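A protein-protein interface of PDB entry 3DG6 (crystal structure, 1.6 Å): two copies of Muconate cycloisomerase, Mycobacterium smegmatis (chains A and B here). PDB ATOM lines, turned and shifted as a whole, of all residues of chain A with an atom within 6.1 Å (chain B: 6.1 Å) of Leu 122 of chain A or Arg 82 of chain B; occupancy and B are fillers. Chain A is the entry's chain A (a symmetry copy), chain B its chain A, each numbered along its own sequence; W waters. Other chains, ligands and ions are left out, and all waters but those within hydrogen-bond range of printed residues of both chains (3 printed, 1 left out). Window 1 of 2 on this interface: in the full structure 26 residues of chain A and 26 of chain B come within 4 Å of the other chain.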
ATOM      1  N   TRP A 107      16.082 -13.217  10.538  1.00  0.00           N
ATOM      2  CA  TRP A 107      14.962 -13.849   9.848  1.00  0.00           C
ATOM      3  C   TRP A 107      13.667 -13.082  10.119  1.00  0.00           C
ATOM      4  O   TRP A 107      12.810 -12.966   9.238  1.00  0.00           O
ATOM      5  CB  TRP A 107      14.789 -15.304  10.301  1.00  0.00           C
ATOM      6  CG  TRP A 107      15.638 -16.309   9.569  1.00  0.00           C
ATOM      7  CD1 TRP A 107      16.873 -16.766   9.932  1.00  0.00           C
ATOM      8  CD2 TRP A 107      15.284 -17.017   8.375  1.00  0.00           C
ATOM      9  NE1 TRP A 107      17.307 -17.721   9.041  1.00  0.00           N
ATOM     10  CE2 TRP A 107      16.350 -17.894   8.075  1.00  0.00           C
ATOM     11  CE3 TRP A 107      14.167 -16.996   7.529  1.00  0.00           C
ATOM     12  CZ2 TRP A 107      16.332 -18.745   6.965  1.00  0.00           C
ATOM     13  CZ3 TRP A 107      14.149 -17.843   6.424  1.00  0.00           C
ATOM     14  CH2 TRP A 107      15.227 -18.705   6.153  1.00  0.00           C
ATOM     15  N   SER A 117       5.784 -14.932   6.843  1.00  0.00           N
ATOM     16  CA  SER A 117       6.107 -15.470   8.158  1.00  0.00           C
ATOM     17  C   SER A 117       7.391 -16.281   8.045  1.00  0.00           C
ATOM     18  O   SER A 117       7.721 -16.797   6.975  1.00  0.00           O
ATOM     19  CB  SER A 117       4.991 -16.387   8.658  1.00  0.00           C
ATOM     20  OG  SER A 117       4.861 -17.527   7.822  1.00  0.00           O
ATOM     21  N   VAL A 118       8.120 -16.385   9.149  1.00  0.00           N
ATOM     22  CA  VAL A 118       9.346 -17.170   9.157  1.00  0.00           C
ATOM     23  C   VAL A 118       8.978 -18.613   8.818  1.00  0.00           C
ATOM     24  O   VAL A 118       9.658 -19.268   8.031  1.00  0.00           O
ATOM     25  CB  VAL A 118      10.028 -17.114  10.544  1.00  0.00           C
ATOM     26  CG1 VAL A 118      11.139 -18.153  10.633  1.00  0.00           C
ATOM     27  CG2 VAL A 118      10.600 -15.723  10.770  1.00  0.00           C
ATOM     28  N   SER A 119       7.885 -19.094   9.401  1.00  0.00           N
ATOM     29  CA  SER A 119       7.435 -20.458   9.158  1.00  0.00           C
ATOM     30  C   SER A 119       7.277 -20.780   7.675  1.00  0.00           C
ATOM     31  O   SER A 119       7.800 -21.786   7.200  1.00  0.00           O
ATOM     32  CB  SER A 119       6.110 -20.724   9.872  1.00  0.00           C
ATOM     33  OG  SER A 119       5.656 -22.039   9.596  1.00  0.00           O
ATOM     34  N   GLU A 120       6.560 -19.935   6.939  1.00  0.00           N
ATOM     35  CA  GLU A 120       6.367 -20.212   5.523  1.00  0.00           C
ATOM     36  C   GLU A 120       7.655 -20.086   4.717  1.00  0.00           C
ATOM     37  O   GLU A 120       7.882 -20.863   3.790  1.00  0.00           O
ATOM     38  CB  GLU A 120       5.258 -19.326   4.935  1.00  0.00           C
ATOM     39  CG  GLU A 120       5.567 -17.851   4.818  1.00  0.00           C
ATOM     40  CD  GLU A 120       4.334 -17.052   4.428  1.00  0.00           C
ATOM     41  OE1 GLU A 120       3.753 -17.328   3.355  1.00  0.00           O
ATOM     42  OE2 GLU A 120       3.939 -16.153   5.196  1.00  0.00           O
ATOM     43  N   MET A 121       8.516 -19.135   5.073  1.00  0.00           N
ATOM     44  CA  MET A 121       9.772 -18.983   4.347  1.00  0.00           C
ATOM     45  C   MET A 121      10.644 -20.228   4.510  1.00  0.00           C
ATOM     46  O   MET A 121      11.358 -20.619   3.587  1.00  0.00           O
ATOM     47  CB  MET A 121      10.538 -17.749   4.835  1.00  0.00           C
ATOM     48  CG  MET A 121       9.884 -16.428   4.453  1.00  0.00           C
ATOM     49  SD  MET A 121      10.956 -15.013   4.773  1.00  0.00           S
ATOM     50  CE  MET A 121      10.954 -15.000   6.551  1.00  0.00           C
ATOM     51  N   LEU A 122      10.569 -20.852   5.682  1.00  0.00           N
ATOM     52  CA  LEU A 122      11.353 -22.050   5.973  1.00  0.00           C
ATOM     53  C   LEU A 122      10.821 -23.323   5.322  1.00  0.00           C
ATOM     54  O   LEU A 122      11.564 -24.289   5.160  1.00  0.00           O
ATOM     55  CB  LEU A 122      11.452 -22.265   7.488  1.00  0.00           C
ATOM     56  CG  LEU A 122      12.352 -21.310   8.272  1.00  0.00           C
ATOM     57  CD1 LEU A 122      12.184 -21.551   9.764  1.00  0.00           C
ATOM     58  CD2 LEU A 122      13.807 -21.517   7.854  1.00  0.00           C
ATOM     59  N   GLY A 123       9.543 -23.333   4.952  1.00  0.00           N
ATOM     60  CA  GLY A 123       8.978 -24.520   4.330  1.00  0.00           C
ATOM     61  C   GLY A 123       7.462 -24.596   4.383  1.00  0.00           C
ATOM     62  O   GLY A 123       6.838 -25.242   3.541  1.00  0.00           O
ATOM     63  N   GLY A 124       6.880 -23.953   5.392  1.00  0.00           N
ATOM     64  CA  GLY A 124       5.432 -23.922   5.546  1.00  0.00           C
ATOM     65  C   GLY A 124       4.686 -25.247   5.496  1.00  0.00           C
ATOM     66  O   GLY A 124       3.608 -25.327   4.902  1.00  0.00           O
ATOM     67  N   PHE A 272      17.500 -20.480  13.202  1.00  0.00           N
ATOM     68  CA  PHE A 272      16.760 -21.038  12.076  1.00  0.00           C
ATOM     69  C   PHE A 272      17.725 -21.576  11.024  1.00  0.00           C
ATOM     70  O   PHE A 272      17.529 -22.668  10.492  1.00  0.00           O
ATOM     71  CB  PHE A 272      15.816 -19.995  11.454  1.00  0.00           C
ATOM     72  CG  PHE A 272      14.799 -19.444  12.419  1.00  0.00           C
ATOM     73  CD1 PHE A 272      14.166 -20.276  13.338  1.00  0.00           C
ATOM     74  CD2 PHE A 272      14.474 -18.089  12.408  1.00  0.00           C
ATOM     75  CE1 PHE A 272      13.227 -19.770  14.235  1.00  0.00           C
ATOM     76  CE2 PHE A 272      13.535 -17.571  13.300  1.00  0.00           C
ATOM     77  CZ  PHE A 272      12.911 -18.409  14.215  1.00  0.00           C
ATOM     78  N   THR A 273      18.778 -20.818  10.726  1.00  0.00           N
ATOM     79  CA  THR A 273      19.757 -21.271   9.750  1.00  0.00           C
ATOM     80  C   THR A 273      20.445 -22.526  10.291  1.00  0.00           C
ATOM     81  O   THR A 273      20.559 -23.530   9.589  1.00  0.00           O
ATOM     82  CB  THR A 273      20.797 -20.172   9.469  1.00  0.00           C
ATOM     83  OG1 THR A 273      20.123 -19.019   8.947  1.00  0.00           O
ATOM     84  CG2 THR A 273      21.827 -20.650   8.453  1.00  0.00           C
ATOM     85  N   THR A 276      18.069 -25.584  10.603  1.00  0.00           N
ATOM     86  CA  THR A 276      17.785 -26.244   9.333  1.00  0.00           C
ATOM     87  C   THR A 276      18.918 -27.240   9.072  1.00  0.00           C
ATOM     88  O   THR A 276      18.691 -28.334   8.557  1.00  0.00           O
ATOM     89  CB  THR A 276      17.698 -25.231   8.168  1.00  0.00           C
ATOM     90  OG1 THR A 276      16.668 -24.270   8.448  1.00  0.00           O
ATOM     91  CG2 THR A 276      17.359 -25.944   6.864  1.00  0.00           C
ATOM     92  N   SER A 306       7.793 -21.310  15.018  1.00  0.00           N
ATOM     93  CA  SER A 306       8.040 -20.863  13.650  1.00  0.00           C
ATOM     94  C   SER A 306       8.824 -21.936  12.898  1.00  0.00           C
ATOM     95  O   SER A 306       8.507 -22.267  11.757  1.00  0.00           O
ATOM     96  CB  SER A 306       8.843 -19.556  13.635  1.00  0.00           C
ATOM     97  OG  SER A 306       8.058 -18.457  14.063  1.00  0.00           O
ATOM     98  N   PHE A 307       9.848 -22.487  13.542  1.00  0.00           N
ATOM     99  CA  PHE A 307      10.664 -23.517  12.908  1.00  0.00           C
ATOM    100  C   PHE A 307       9.974 -24.881  12.856  1.00  0.00           C
ATOM    101  O   PHE A 307       9.948 -25.537  11.812  1.00  0.00           O
ATOM    102  CB  PHE A 307      12.001 -23.672  13.642  1.00  0.00           C
ATOM    103  CG  PHE A 307      12.947 -24.611  12.957  1.00  0.00           C
ATOM    104  CD1 PHE A 307      13.753 -24.166  11.911  1.00  0.00           C
ATOM    105  CD2 PHE A 307      12.980 -25.960  13.303  1.00  0.00           C
ATOM    106  CE1 PHE A 307      14.575 -25.050  11.215  1.00  0.00           C
ATOM    107  CE2 PHE A 307      13.799 -26.854  12.613  1.00  0.00           C
ATOM    108  CZ  PHE A 307      14.596 -26.398  11.564  1.00  0.00           C
ATOM    109  N   ALA A 310       7.441 -25.551  10.133  1.00  0.00           N
ATOM    110  CA  ALA A 310       7.949 -25.512   8.768  1.00  0.00           C
ATOM    111  C   ALA A 310       8.219 -26.875   8.141  1.00  0.00           C
ATOM    112  O   ALA A 310       8.154 -27.017   6.916  1.00  0.00           O
ATOM    113  CB  ALA A 310       9.220 -24.664   8.718  1.00  0.00           C
ATOM    114  N   PHE A 311       8.501 -27.868   8.982  1.00  0.00           N
ATOM    115  CA  PHE A 311       8.832 -29.213   8.517  1.00  0.00           C
ATOM    116  C   PHE A 311       7.949 -30.319   9.080  1.00  0.00           C
ATOM    117  O   PHE A 311       7.434 -30.219  10.196  1.00  0.00           O
ATOM    118  CB  PHE A 311      10.286 -29.526   8.880  1.00  0.00           C
ATOM    119  CG  PHE A 311      11.276 -28.560   8.298  1.00  0.00           C
ATOM    120  CD1 PHE A 311      11.696 -28.690   6.978  1.00  0.00           C
ATOM    121  CD2 PHE A 311      11.776 -27.511   9.064  1.00  0.00           C
ATOM    122  CE1 PHE A 311      12.603 -27.789   6.424  1.00  0.00           C
ATOM    123  CE2 PHE A 311      12.685 -26.600   8.520  1.00  0.00           C
ATOM    124  CZ  PHE A 311      13.097 -26.742   7.199  1.00  0.00           C
ATOM    125  N   THR B  78       0.841 -22.780  -2.294  1.00  0.00           N
ATOM    126  CA  THR B  78       1.463 -21.479  -2.509  1.00  0.00           C
ATOM    127  C   THR B  78       2.958 -21.708  -2.656  1.00  0.00           C
ATOM    128  O   THR B  78       3.458 -22.799  -2.372  1.00  0.00           O
ATOM    129  CB  THR B  78       1.253 -20.519  -1.323  1.00  0.00           C
ATOM    130  OG1 THR B  78       2.021 -20.970  -0.204  1.00  0.00           O
ATOM    131  CG2 THR B  78      -0.219 -20.453  -0.936  1.00  0.00           C
ATOM    132  N   LEU B  79       3.670 -20.677  -3.095  1.00  0.00           N
ATOM    133  CA  LEU B  79       5.110 -20.783  -3.275  1.00  0.00           C
ATOM    134  C   LEU B  79       5.844 -20.837  -1.938  1.00  0.00           C
ATOM    135  O   LEU B  79       7.062 -21.019  -1.904  1.00  0.00           O
ATOM    136  CB  LEU B  79       5.621 -19.614  -4.125  1.00  0.00           C
ATOM    137  CG  LEU B  79       5.030 -19.536  -5.540  1.00  0.00           C
ATOM    138  CD1 LEU B  79       5.613 -18.340  -6.272  1.00  0.00           C
ATOM    139  CD2 LEU B  79       5.327 -20.817  -6.306  1.00  0.00           C
ATOM    140  N   THR B  80       5.107 -20.683  -0.838  1.00  0.00           N
ATOM    141  CA  THR B  80       5.713 -20.749   0.489  1.00  0.00           C
ATOM    142  C   THR B  80       5.232 -21.980   1.260  1.00  0.00           C
ATOM    143  O   THR B  80       5.093 -21.966   2.490  1.00  0.00           O
ATOM    144  CB  THR B  80       5.447 -19.465   1.313  1.00  0.00           C
ATOM    145  OG1 THR B  80       4.043 -19.181   1.340  1.00  0.00           O
ATOM    146  CG2 THR B  80       6.198 -18.284   0.701  1.00  0.00           C
ATOM    147  N   GLU B  81       4.971 -23.042   0.506  1.00  0.00           N
ATOM    148  CA  GLU B  81       4.568 -24.326   1.061  1.00  0.00           C
ATOM    149  C   GLU B  81       5.468 -25.365   0.400  1.00  0.00           C
ATOM    150  O   GLU B  81       5.022 -26.448   0.024  1.00  0.00           O
ATOM    151  CB  GLU B  81       3.096 -24.626   0.756  1.00  0.00           C
ATOM    152  CG  GLU B  81       2.129 -23.822   1.610  1.00  0.00           C
ATOM    153  CD  GLU B  81       0.678 -24.202   1.381  1.00  0.00           C
ATOM    154  OE1 GLU B  81       0.180 -24.021   0.250  1.00  0.00           O
ATOM    155  OE2 GLU B  81       0.033 -24.684   2.338  1.00  0.00           O
ATOM    156  N   ARG B  82       6.744 -25.019   0.259  1.00  0.00           N
ATOM    157  CA  ARG B  82       7.713 -25.912  -0.370  1.00  0.00           C
ATOM    158  C   ARG B  82       7.809 -27.277   0.294  1.00  0.00           C
ATOM    159  O   ARG B  82       7.999 -28.282  -0.389  1.00  0.00           O
ATOM    160  CB  ARG B  82       9.106 -25.271  -0.402  1.00  0.00           C
ATOM    161  CG  ARG B  82       9.246 -24.131  -1.404  1.00  0.00           C
ATOM    162  CD  ARG B  82      10.659 -23.543  -1.411  1.00  0.00           C
ATOM    163  NE  ARG B  82      11.037 -22.998  -0.110  1.00  0.00           N
ATOM    164  CZ  ARG B  82      11.790 -23.632   0.785  1.00  0.00           C
ATOM    165  NH1 ARG B  82      12.265 -24.846   0.524  1.00  0.00           N
ATOM    166  NH2 ARG B  82      12.056 -23.055   1.950  1.00  0.00           N
ATOM    167  N   GLU B  83       7.690 -27.329   1.617  1.00  0.00           N
ATOM    168  CA  GLU B  83       7.783 -28.613   2.293  1.00  0.00           C
ATOM    169  C   GLU B  83       6.556 -29.485   2.044  1.00  0.00           C
ATOM    170  O   GLU B  83       6.641 -30.708   2.120  1.00  0.00           O
ATOM    171  CB  GLU B  83       8.040 -28.421   3.789  1.00  0.00           C
ATOM    172  CG  GLU B  83       9.485 -28.001   4.098  1.00  0.00           C
ATOM    173  CD  GLU B  83      10.514 -29.021   3.616  1.00  0.00           C
ATOM    174  OE1 GLU B  83      10.297 -30.231   3.832  1.00  0.00           O
ATOM    175  OE2 GLU B  83      11.548 -28.612   3.037  1.00  0.00           O
ATOM    176  N   VAL B  84       5.420 -28.865   1.736  1.00  0.00           N
ATOM    177  CA  VAL B  84       4.222 -29.638   1.428  1.00  0.00           C
ATOM    178  C   VAL B  84       4.452 -30.246   0.043  1.00  0.00           C
ATOM    179  O   VAL B  84       4.188 -31.424  -0.186  1.00  0.00           O
ATOM    180  CB  VAL B  84       2.951 -28.751   1.386  1.00  0.00           C
ATOM    181  CG1 VAL B  84       1.741 -29.599   1.008  1.00  0.00           C
ATOM    182  CG2 VAL B  84       2.723 -28.095   2.742  1.00  0.00           C
ATOM    183  N   ALA B  85       4.956 -29.435  -0.880  1.00  0.00           N
ATOM    184  CA  ALA B  85       5.232 -29.906  -2.233  1.00  0.00           C
ATOM    185  C   ALA B  85       6.288 -31.010  -2.185  1.00  0.00           C
ATOM    186  O   ALA B  85       6.181 -32.021  -2.878  1.00  0.00           O
ATOM    187  CB  ALA B  85       5.720 -28.747  -3.102  1.00  0.00           C
ATOM    188  N   HIS B  86       7.302 -30.812  -1.350  1.00  0.00           N
ATOM    189  CA  HIS B  86       8.382 -31.782  -1.208  1.00  0.00           C
ATOM    190  C   HIS B  86       7.839 -33.126  -0.725  1.00  0.00           C
ATOM    191  O   HIS B  86       8.159 -34.178  -1.282  1.00  0.00           O
ATOM    192  CB  HIS B  86       9.421 -31.236  -0.223  1.00  0.00           C
ATOM    193  CG  HIS B  86      10.629 -32.105  -0.065  1.00  0.00           C
ATOM    194  ND1 HIS B  86      10.770 -33.004   0.971  1.00  0.00           N
ATOM    195  CD2 HIS B  86      11.752 -32.212  -0.811  1.00  0.00           C
ATOM    196  CE1 HIS B  86      11.930 -33.625   0.855  1.00  0.00           C
ATOM    197  NE2 HIS B  86      12.545 -33.164  -0.217  1.00  0.00           N
ATOM    198  N   THR B  87       6.997 -33.077   0.301  1.00  0.00           N
ATOM    199  CA  THR B  87       6.410 -34.278   0.876  1.00  0.00           C
ATOM    200  C   THR B  87       5.454 -34.980  -0.087  1.00  0.00           C
ATOM    201  O   THR B  87       5.462 -36.210  -0.189  1.00  0.00           O
ATOM    202  CB  THR B  87       5.682 -33.939   2.190  1.00  0.00           C
ATOM    203  OG1 THR B  87       6.594 -33.264   3.068  1.00  0.00           O
ATOM    204  CG2 THR B  87       5.191 -35.204   2.874  1.00  0.00           C
ATOM    205  N   ASP B 103      10.584 -28.113  -8.412  1.00  0.00           N
ATOM    206  CA  ASP B 103      11.079 -27.367  -7.263  1.00  0.00           C
ATOM    207  C   ASP B 103      11.800 -26.086  -7.676  1.00  0.00           C
ATOM    208  O   ASP B 103      11.563 -25.022  -7.109  1.00  0.00           O
ATOM    209  CB  ASP B 103      12.034 -28.230  -6.430  1.00  0.00           C
ATOM    210  CG  ASP B 103      12.577 -27.490  -5.221  1.00  0.00           C
ATOM    211  OD1 ASP B 103      11.789 -27.191  -4.296  1.00  0.00           O
ATOM    212  OD2 ASP B 103      13.793 -27.200  -5.195  1.00  0.00           O
ATOM    213  N   MET B 106       9.488 -23.484  -8.987  1.00  0.00           N
ATOM    214  CA  MET B 106       8.763 -22.870  -7.880  1.00  0.00           C
ATOM    215  C   MET B 106       9.639 -21.797  -7.243  1.00  0.00           C
ATOM    216  O   MET B 106       9.163 -20.711  -6.910  1.00  0.00           O
ATOM    217  CB  MET B 106       8.378 -23.916  -6.827  1.00  0.00           C
ATOM    218  CG  MET B 106       7.217 -24.799  -7.236  1.00  0.00           C
ATOM    219  SD  MET B 106       6.767 -25.980  -5.940  1.00  0.00           S
ATOM    220  CE  MET B 106       6.317 -24.899  -4.625  1.00  0.00           C
ATOM    221  N   TRP B 107      10.921 -22.103  -7.067  1.00  0.00           N
ATOM    222  CA  TRP B 107      11.850 -21.137  -6.490  1.00  0.00           C
ATOM    223  C   TRP B 107      12.022 -19.938  -7.423  1.00  0.00           C
ATOM    224  O   TRP B 107      12.162 -18.800  -6.965  1.00  0.00           O
ATOM    225  CB  TRP B 107      13.221 -21.777  -6.236  1.00  0.00           C
ATOM    226  CG  TRP B 107      13.359 -22.498  -4.921  1.00  0.00           C
ATOM    227  CD1 TRP B 107      13.144 -23.827  -4.682  1.00  0.00           C
ATOM    228  CD2 TRP B 107      13.795 -21.933  -3.679  1.00  0.00           C
ATOM    229  NE1 TRP B 107      13.427 -24.124  -3.369  1.00  0.00           N
ATOM    230  CE2 TRP B 107      13.828 -22.980  -2.731  1.00  0.00           C
ATOM    231  CE3 TRP B 107      14.162 -20.643  -3.275  1.00  0.00           C
ATOM    232  CZ2 TRP B 107      14.216 -22.777  -1.402  1.00  0.00           C
ATOM    233  CZ3 TRP B 107      14.548 -20.439  -1.953  1.00  0.00           C
ATOM    234  CH2 TRP B 107      14.571 -21.503  -1.033  1.00  0.00           C
ATOM    235  N   LEU B 110       9.032 -17.849  -6.965  1.00  0.00           N
ATOM    236  CA  LEU B 110       9.098 -17.203  -5.661  1.00  0.00           C
ATOM    237  C   LEU B 110      10.026 -15.990  -5.729  1.00  0.00           C
ATOM    238  O   LEU B 110       9.681 -14.906  -5.266  1.00  0.00           O
ATOM    239  CB  LEU B 110       9.613 -18.188  -4.606  1.00  0.00           C
ATOM    240  CG  LEU B 110       9.755 -17.638  -3.184  1.00  0.00           C
ATOM    241  CD1 LEU B 110       8.391 -17.232  -2.646  1.00  0.00           C
ATOM    242  CD2 LEU B 110      10.388 -18.695  -2.290  1.00  0.00           C
ATOM    243  N   THR B 273      15.531 -27.283  -2.944  1.00  0.00           N
ATOM    244  CA  THR B 273      15.095 -27.780  -1.648  1.00  0.00           C
ATOM    245  C   THR B 273      15.860 -29.066  -1.331  1.00  0.00           C
ATOM    246  O   THR B 273      16.407 -29.218  -0.240  1.00  0.00           O
ATOM    247  CB  THR B 273      13.579 -28.046  -1.648  1.00  0.00           C
ATOM    248  OG1 THR B 273      12.893 -26.819  -1.928  1.00  0.00           O
ATOM    249  CG2 THR B 273      13.124 -28.574  -0.293  1.00  0.00           C
HETATM  250  O   HOH W   1       0.723 -25.728   4.687  1.00  0.00           O
HETATM  251  O   HOH W   2      14.149 -24.064   4.346  1.00  0.00           O
HETATM  252  O   HOH W   3      12.950 -26.327   2.922  1.00  0.00           O
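Among the printed residues, merely in contact across the chains: Gly 123 of chain A with Thr 80 of chain B (3.9 Å), Gly 123 of chain A with Glu 81 of chain B (3.4 Å), Gly 124 of chain A with Thr 80 of chain B (3.6 Å), Gly 124 of chain A with Glu 81 of chain B (3.9 Å), Gly 124 of chain A with Val 84 of chain B (3.6 Å), Ala 310 of chain A with Glu 83 of chain B (3.3 Å) and Phe 311 of chain A with Glu 83 of chain B (3.6 Å).
Positions printed for both chains: 107 and 273. Of the 12 pairs that touch across the chains among the printed residues, none has its exchanged pair printed and touching as well.
The side-chain hydroxyl (OG1) of Thr 78 of chain B is in hydrogen-bond range of the side-chain hydroxyl (OG1) of Thr 80 of chain B, at 3.1 Å. The side-chain carboxylate of Glu 81 of chain B lies within hydrogen-bond range of the backbone NH of Thr 78 of chain B. O of Ser 119 of chain A lies within hydrogen-bond range of N of Gly 124 of chain A. OG1 of Thr 87 of chain B lies within hydrogen-bond range of O of Glu 83 of chain B (2.7 Å). OE2 of Glu 120 of chain A is in hydrogen-bond range of N of Ser 117 of chain A, at 2.8 Å. NH1 of Arg 82 of chain B sits at hydrogen-bond distance from OG1 of Thr 273 of chain B.
Of the 15 printed residues of chain B, 5 touch a printed residue of chain A. Printed residues of chain B that touch a printed residue of chain A: Thr 80, Glu 81, Arg 82, Glu 83 and Val 84.
The backbone NH (N) of Arg 82 of chain B is in hydrogen-bond range of the backbone carbonyl oxygen (O) of Gly 123 of chain A. The side-chain hydroxyl (OG1) of Thr 80 of chain B lies within hydrogen-bond range of the side-chain carboxylate (OE1) of Glu 120 of chain A (2.8 Å). O of Gly 123 of chain A is in hydrogen-bond range of N of Glu 83 of chain B (3.0 Å). The backbone carbonyl oxygen (O) of Leu 122 of chain A sits at hydrogen-bond distance from the guanidinium group (NH2) of Arg 82 of chain B (3.5 Å). O of Met 121 of chain A is in hydrogen-bond range of NH2 of Arg 82 of chain B, 3.0 Å away.
Water W1 lies within hydrogen-bond range of OE2 of Glu 81 of chain B (2.7 Å) and O of Gly 124 of chain A (2.9 Å). Water W3 lies within hydrogen-bond range of OE2 of Glu 83 of chain B, NH1 of Arg 82 of chain B and O of Leu 122 of chain A. Water W2 lies within hydrogen-bond range of O of Leu 122 of chain A (2.7 Å) and NH2 of Arg 82 of chain B (3.3 Å).
Leu 122 of chain A touches just one residue of chain B: Arg 82. Of the printed residues of chain B, Gly 123 of chain A touches Thr 80, Glu 81, Arg 82 and Glu 83. Printed residues of chain B within 4 Å of Gly 124 of chain A: Thr 80 (3.6 Å), Glu 81 (3.9 Å) and Val 84 (3.6 Å). Printed residues of chain A within 4 Å of Thr 80 of chain B: Glu 120 (2.8 Å), Gly 123 (3.9 Å) and Gly 124 (3.6 Å). Arg 82 of chain B touches just these residues of chain A: Met 121, Leu 122 and Gly 123. Of the printed residues of chain A, Val 84 of chain B touches Gly 124. The nearest residue of chain B that does not touch Leu 122 of chain A is Glu 83 of chain B (4.4 Å).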
